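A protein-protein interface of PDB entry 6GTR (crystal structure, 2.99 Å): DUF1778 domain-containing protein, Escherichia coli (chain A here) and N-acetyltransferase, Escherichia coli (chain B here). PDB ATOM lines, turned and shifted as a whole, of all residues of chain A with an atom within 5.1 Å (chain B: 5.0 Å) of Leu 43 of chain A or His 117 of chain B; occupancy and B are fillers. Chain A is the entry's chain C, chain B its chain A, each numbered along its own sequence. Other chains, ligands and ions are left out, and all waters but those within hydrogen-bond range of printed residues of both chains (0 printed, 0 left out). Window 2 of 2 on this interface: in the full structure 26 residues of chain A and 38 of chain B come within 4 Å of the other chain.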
ATOM      1  N   ALA A  39       6.738   6.419  21.614  1.00  0.00           N
ATOM      2  CA  ALA A  39       7.599   5.260  21.402  1.00  0.00           C
ATOM      3  C   ALA A  39       8.950   5.710  20.831  1.00  0.00           C
ATOM      4  O   ALA A  39       9.979   5.258  21.316  1.00  0.00           O
ATOM      5  CB  ALA A  39       6.924   4.265  20.472  1.00  0.00           C
ATOM      6  N   ALA A  40       8.948   6.663  19.881  1.00  0.00           N
ATOM      7  CA  ALA A  40      10.171   7.222  19.306  1.00  0.00           C
ATOM      8  C   ALA A  40      10.992   8.045  20.334  1.00  0.00           C
ATOM      9  O   ALA A  40      12.229   8.071  20.234  1.00  0.00           O
ATOM     10  CB  ALA A  40       9.842   8.067  18.090  1.00  0.00           C
ATOM     11  N   LYS A  41      10.311   8.707  21.313  1.00  0.00           N
ATOM     12  CA  LYS A  41      10.979   9.484  22.370  1.00  0.00           C
ATOM     13  C   LYS A  41      11.706   8.529  23.345  1.00  0.00           C
ATOM     14  O   LYS A  41      12.765   8.884  23.877  1.00  0.00           O
ATOM     15  CB  LYS A  41       9.980  10.391  23.111  1.00  0.00           C
ATOM     16  CG  LYS A  41      10.623  11.467  24.000  1.00  0.00           C
ATOM     17  CD  LYS A  41      10.688  11.054  25.482  1.00  0.00           C
ATOM     18  CE  LYS A  41      11.339  12.102  26.354  1.00  0.00           C
ATOM     19  NZ  LYS A  41      11.274  11.744  27.798  1.00  0.00           N
ATOM     20  N   ARG A  42      11.115   7.319  23.557  1.00  0.00           N
ATOM     21  CA  ARG A  42      11.670   6.273  24.417  1.00  0.00           C
ATOM     22  C   ARG A  42      12.940   5.721  23.789  1.00  0.00           C
ATOM     23  O   ARG A  42      13.932   5.540  24.489  1.00  0.00           O
ATOM     24  CB  ARG A  42      10.648   5.151  24.627  1.00  0.00           C
ATOM     25  CG  ARG A  42       9.419   5.604  25.397  1.00  0.00           C
ATOM     26  CD  ARG A  42       9.308   4.887  26.718  1.00  0.00           C
ATOM     27  NE  ARG A  42       8.966   3.483  26.514  1.00  0.00           N
ATOM     28  CZ  ARG A  42       8.782   2.610  27.491  1.00  0.00           C
ATOM     29  NH1 ARG A  42       8.913   2.983  28.759  1.00  0.00           N
ATOM     30  NH2 ARG A  42       8.472   1.356  27.212  1.00  0.00           N
ATOM     31  N   LEU A  43      12.911   5.499  22.449  1.00  0.00           N
ATOM     32  CA  LEU A  43      13.990   5.009  21.588  1.00  0.00           C
ATOM     33  C   LEU A  43      15.194   5.968  21.583  1.00  0.00           C
ATOM     34  O   LEU A  43      16.342   5.524  21.515  1.00  0.00           O
ATOM     35  CB  LEU A  43      13.439   4.809  20.164  1.00  0.00           C
ATOM     36  CG  LEU A  43      14.316   4.077  19.150  1.00  0.00           C
ATOM     37  CD1 LEU A  43      14.717   2.663  19.648  1.00  0.00           C
ATOM     38  CD2 LEU A  43      13.641   4.036  17.790  1.00  0.00           C
ATOM     39  N   GLN A  44      14.918   7.278  21.677  1.00  0.00           N
ATOM     40  CA  GLN A  44      15.921   8.335  21.747  1.00  0.00           C
ATOM     41  C   GLN A  44      16.783   8.188  23.005  1.00  0.00           C
ATOM     42  O   GLN A  44      18.006   8.261  22.896  1.00  0.00           O
ATOM     43  CB  GLN A  44      15.253   9.720  21.736  1.00  0.00           C
ATOM     44  CG  GLN A  44      14.838  10.221  20.355  1.00  0.00           C
ATOM     45  CD  GLN A  44      14.914  11.729  20.304  1.00  0.00           C
ATOM     46  OE1 GLN A  44      15.924  12.314  19.887  1.00  0.00           O
ATOM     47  NE2 GLN A  44      13.858  12.398  20.748  1.00  0.00           N
ATOM     48  N   GLY A  45      16.145   7.951  24.161  1.00  0.00           N
ATOM     49  CA  GLY A  45      16.815   7.807  25.454  1.00  0.00           C
ATOM     50  C   GLY A  45      17.524   6.489  25.712  1.00  0.00           C
ATOM     51  O   GLY A  45      18.049   6.276  26.809  1.00  0.00           O
ATOM     52  N   MET A  46      17.557   5.595  24.712  1.00  0.00           N
ATOM     53  CA  MET A  46      18.184   4.276  24.813  1.00  0.00           C
ATOM     54  C   MET A  46      19.495   4.213  24.027  1.00  0.00           C
ATOM     55  O   MET A  46      20.346   5.092  24.162  1.00  0.00           O
ATOM     56  CB  MET A  46      17.219   3.193  24.310  1.00  0.00           C
ATOM     57  CG  MET A  46      16.012   3.005  25.192  1.00  0.00           C
ATOM     58  SD  MET A  46      14.921   1.716  24.575  1.00  0.00           S
ATOM     59  CE  MET A  46      15.803   0.263  25.114  1.00  0.00           C
ATOM     60  N   ILE B   9      17.737  -2.643  23.248  1.00  0.00           N
ATOM     61  CA  ILE B   9      17.245  -3.290  22.019  1.00  0.00           C
ATOM     62  C   ILE B   9      18.434  -3.493  21.080  1.00  0.00           C
ATOM     63  O   ILE B   9      19.104  -2.520  20.735  1.00  0.00           O
ATOM     64  CB  ILE B   9      16.073  -2.531  21.327  1.00  0.00           C
ATOM     65  CG1 ILE B   9      14.926  -2.212  22.308  1.00  0.00           C
ATOM     66  CG2 ILE B   9      15.557  -3.318  20.129  1.00  0.00           C
ATOM     67  CD1 ILE B   9      14.122  -0.998  21.933  1.00  0.00           C
ATOM     68  N   GLU B  10      18.701  -4.746  20.669  1.00  0.00           N
ATOM     69  CA  GLU B  10      19.847  -5.068  19.814  1.00  0.00           C
ATOM     70  C   GLU B  10      19.529  -6.174  18.828  1.00  0.00           C
ATOM     71  O   GLU B  10      18.585  -6.917  19.041  1.00  0.00           O
ATOM     72  CB  GLU B  10      21.068  -5.460  20.687  1.00  0.00           C
ATOM     73  CG  GLU B  10      20.998  -6.855  21.303  1.00  0.00           C
ATOM     74  CD  GLU B  10      22.023  -7.198  22.368  1.00  0.00           C
ATOM     75  OE1 GLU B  10      22.461  -8.374  22.421  1.00  0.00           O
ATOM     76  OE2 GLU B  10      22.369  -6.296  23.166  1.00  0.00           O
ATOM     77  N   TYR B  50      15.599  -9.459  16.399  1.00  0.00           N
ATOM     78  CA  TYR B  50      15.945  -8.326  17.263  1.00  0.00           C
ATOM     79  C   TYR B  50      15.406  -8.601  18.647  1.00  0.00           C
ATOM     80  O   TYR B  50      14.290  -9.100  18.770  1.00  0.00           O
ATOM     81  CB  TYR B  50      15.391  -7.030  16.686  1.00  0.00           C
ATOM     82  CG  TYR B  50      16.182  -6.540  15.496  1.00  0.00           C
ATOM     83  CD1 TYR B  50      15.974  -7.074  14.225  1.00  0.00           C
ATOM     84  CD2 TYR B  50      17.159  -5.555  15.641  1.00  0.00           C
ATOM     85  CE1 TYR B  50      16.724  -6.648  13.128  1.00  0.00           C
ATOM     86  CE2 TYR B  50      17.902  -5.107  14.548  1.00  0.00           C
ATOM     87  CZ  TYR B  50      17.691  -5.667  13.294  1.00  0.00           C
ATOM     88  OH  TYR B  50      18.413  -5.218  12.213  1.00  0.00           O
ATOM     89  N   TYR B  65      11.421  -9.190  18.047  1.00  0.00           N
ATOM     90  CA  TYR B  65      10.761  -8.908  16.783  1.00  0.00           C
ATOM     91  C   TYR B  65      11.572  -9.526  15.673  1.00  0.00           C
ATOM     92  O   TYR B  65      12.742  -9.840  15.866  1.00  0.00           O
ATOM     93  CB  TYR B  65      10.356  -7.425  16.550  1.00  0.00           C
ATOM     94  CG  TYR B  65      11.446  -6.465  16.131  1.00  0.00           C
ATOM     95  CD1 TYR B  65      11.842  -6.371  14.803  1.00  0.00           C
ATOM     96  CD2 TYR B  65      11.949  -5.522  17.023  1.00  0.00           C
ATOM     97  CE1 TYR B  65      12.796  -5.443  14.396  1.00  0.00           C
ATOM     98  CE2 TYR B  65      12.890  -4.573  16.622  1.00  0.00           C
ATOM     99  CZ  TYR B  65      13.318  -4.547  15.309  1.00  0.00           C
ATOM    100  OH  TYR B  65      14.269  -3.650  14.898  1.00  0.00           O
ATOM    101  N   THR B 113       7.694   0.759  21.280  1.00  0.00           N
ATOM    102  CA  THR B 113       9.119   1.131  21.186  1.00  0.00           C
ATOM    103  C   THR B 113       9.843   0.147  20.271  1.00  0.00           C
ATOM    104  O   THR B 113      10.720   0.560  19.504  1.00  0.00           O
ATOM    105  CB  THR B 113       9.808   1.189  22.573  1.00  0.00           C
ATOM    106  OG1 THR B 113       8.984   1.860  23.543  1.00  0.00           O
ATOM    107  CG2 THR B 113      11.186   1.855  22.507  1.00  0.00           C
ATOM    108  N   LEU B 114       9.465  -1.154  20.342  1.00  0.00           N
ATOM    109  CA  LEU B 114      10.031  -2.195  19.487  1.00  0.00           C
ATOM    110  C   LEU B 114       9.641  -1.942  18.023  1.00  0.00           C
ATOM    111  O   LEU B 114      10.493  -2.044  17.151  1.00  0.00           O
ATOM    112  CB  LEU B 114       9.642  -3.620  19.953  1.00  0.00           C
ATOM    113  CG  LEU B 114      10.373  -4.265  21.170  1.00  0.00           C
ATOM    114  CD1 LEU B 114      10.298  -5.782  21.088  1.00  0.00           C
ATOM    115  CD2 LEU B 114      11.846  -3.951  21.187  1.00  0.00           C
ATOM    116  N   VAL B 115       8.387  -1.534  17.767  1.00  0.00           N
ATOM    117  CA  VAL B 115       7.899  -1.197  16.422  1.00  0.00           C
ATOM    118  C   VAL B 115       8.641   0.065  15.921  1.00  0.00           C
ATOM    119  O   VAL B 115       8.988   0.150  14.751  1.00  0.00           O
ATOM    120  CB  VAL B 115       6.345  -1.044  16.396  1.00  0.00           C
ATOM    121  CG1 VAL B 115       5.849  -0.525  15.044  1.00  0.00           C
ATOM    122  CG2 VAL B 115       5.662  -2.366  16.737  1.00  0.00           C
ATOM    123  N   ALA B 116       8.916   1.016  16.828  1.00  0.00           N
ATOM    124  CA  ALA B 116       9.639   2.246  16.515  1.00  0.00           C
ATOM    125  C   ALA B 116      11.092   1.919  16.183  1.00  0.00           C
ATOM    126  O   ALA B 116      11.632   2.470  15.224  1.00  0.00           O
ATOM    127  CB  ALA B 116       9.551   3.222  17.680  1.00  0.00           C
ATOM    128  N   HIS B 117      11.705   0.973  16.933  1.00  0.00           N
ATOM    129  CA  HIS B 117      13.064   0.496  16.669  1.00  0.00           C
ATOM    130  C   HIS B 117      13.078  -0.205  15.298  1.00  0.00           C
ATOM    131  O   HIS B 117      13.972   0.048  14.491  1.00  0.00           O
ATOM    132  CB  HIS B 117      13.550  -0.433  17.784  1.00  0.00           C
ATOM    133  CG  HIS B 117      14.957  -0.899  17.583  1.00  0.00           C
ATOM    134  ND1 HIS B 117      15.241  -2.025  16.837  1.00  0.00           N
ATOM    135  CD2 HIS B 117      16.117  -0.376  18.042  1.00  0.00           C
ATOM    136  CE1 HIS B 117      16.555  -2.150  16.858  1.00  0.00           C
ATOM    137  NE2 HIS B 117      17.126  -1.194  17.593  1.00  0.00           N
ATOM    138  N   ALA B 118      12.039  -1.019  15.023  1.00  0.00           N
ATOM    139  CA  ALA B 118      11.841  -1.693  13.750  1.00  0.00           C
ATOM    140  C   ALA B 118      11.823  -0.653  12.643  1.00  0.00           C
ATOM    141  O   ALA B 118      12.611  -0.767  11.698  1.00  0.00           O
ATOM    142  CB  ALA B 118      10.537  -2.463  13.759  1.00  0.00           C
ATOM    143  N   MET B 119      11.004   0.414  12.810  1.00  0.00           N
ATOM    144  CA  MET B 119      10.880   1.509  11.845  1.00  0.00           C
ATOM    145  C   MET B 119      12.185   2.240  11.588  1.00  0.00           C
ATOM    146  O   MET B 119      12.441   2.615  10.450  1.00  0.00           O
ATOM    147  CB  MET B 119       9.793   2.484  12.258  1.00  0.00           C
ATOM    148  CG  MET B 119       8.394   1.952  12.050  1.00  0.00           C
ATOM    149  SD  MET B 119       7.246   3.159  12.706  1.00  0.00           S
ATOM    150  CE  MET B 119       5.780   2.291  12.564  1.00  0.00           C
ATOM    151  N   ASN B 120      13.043   2.379  12.604  1.00  0.00           N
ATOM    152  CA  ASN B 120      14.343   3.031  12.420  1.00  0.00           C
ATOM    153  C   ASN B 120      15.328   2.163  11.600  1.00  0.00           C
ATOM    154  O   ASN B 120      16.178   2.702  10.879  1.00  0.00           O
ATOM    155  CB  ASN B 120      14.934   3.453  13.759  1.00  0.00           C
ATOM    156  CG  ASN B 120      16.178   4.290  13.647  1.00  0.00           C
ATOM    157  OD1 ASN B 120      16.200   5.379  13.032  1.00  0.00           O
ATOM    158  ND2 ASN B 120      17.240   3.792  14.248  1.00  0.00           N
ATOM    159  N   VAL B 121      15.184   0.826  11.692  1.00  0.00           N
ATOM    160  CA  VAL B 121      16.006  -0.134  10.946  1.00  0.00           C
ATOM    161  C   VAL B 121      15.588  -0.074   9.460  1.00  0.00           C
ATOM    162  O   VAL B 121      16.439   0.100   8.584  1.00  0.00           O
ATOM    163  CB  VAL B 121      15.876  -1.567  11.522  1.00  0.00           C
ATOM    164  CG1 VAL B 121      16.587  -2.582  10.634  1.00  0.00           C
ATOM    165  CG2 VAL B 121      16.375  -1.648  12.966  1.00  0.00           C
ATOM    166  N   PHE B 174      11.078  10.499  12.747  1.00  0.00           N
ATOM    167  CA  PHE B 174      12.386  10.798  13.263  1.00  0.00           C
ATOM    168  C   PHE B 174      12.985  12.011  12.623  1.00  0.00           C
ATOM    169  O   PHE B 174      14.172  12.196  12.669  1.00  0.00           O
ATOM    170  CB  PHE B 174      13.327   9.629  13.013  1.00  0.00           C
ATOM    171  CG  PHE B 174      12.819   8.334  13.529  1.00  0.00           C
ATOM    172  CD1 PHE B 174      12.781   8.086  14.862  1.00  0.00           C
ATOM    173  CD2 PHE B 174      12.381   7.377  12.676  1.00  0.00           C
ATOM    174  CE1 PHE B 174      12.296   6.913  15.340  1.00  0.00           C
ATOM    175  CE2 PHE B 174      11.897   6.199  13.142  1.00  0.00           C
ATOM    176  CZ  PHE B 174      11.852   5.968  14.475  1.00  0.00           C
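Thr 113 of chain B touches Ala 39 of chain A (N to CB, 3.7 Å).
Ala 116 of chain B touches Ala 39 of chain A (CB to CB, 3.97 Å).
CB of Ala 40 of chain A touches CE1 of Phe 174 of chain B, at 3.9 Å.
Ala 116 of chain B touches Leu 43 of chain A (O to CD2, 3.6 Å).
Leu 43 of chain A touches His 117 of chain B.
Ile 9 of chain B touches Met 46 of chain A (CD1 to CE, 3.8 Å).
OH of Tyr 65 of chain B sits at hydrogen-bond distance from ND1 of His 117 of chain B, at 2.7 Å.
Printed residues of chain B within 4 Å of Leu 43 of chain A: Ala 116 and His 117.
His 117 of chain B touches just one residue of chain A: Leu 43.
Of the printed residues of chain B, Met 46 of chain A touches Ile 9 (3.8 Å).
Printed residues of chain B within 4 Å of Ala 39 of chain A: Thr 113 and Ala 116.
Val 121 of chain B touches none of the printed residues of chain A.
Lys 41 of chain A touches none of the printed residues of chain B.
OG1 of Thr 113 of chain B lies within hydrogen-bond range of NE of Arg 42 of chain A, at 3.4 Å.
Hydrophobic or aromatic side chains of chain A within 4 Å of the printed part of chain B: Ala 39, Ala 40, Leu 43 and Met 46.
Of the 14 printed residues of chain B, 5 touch a printed residue of chain A.
Among the printed residues, 7 pairs touch across the chains.
Among the printed residues, no Asp or Glu carboxylate lies within 4 Å of a Lys or Arg side-chain nitrogen of the other chain.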
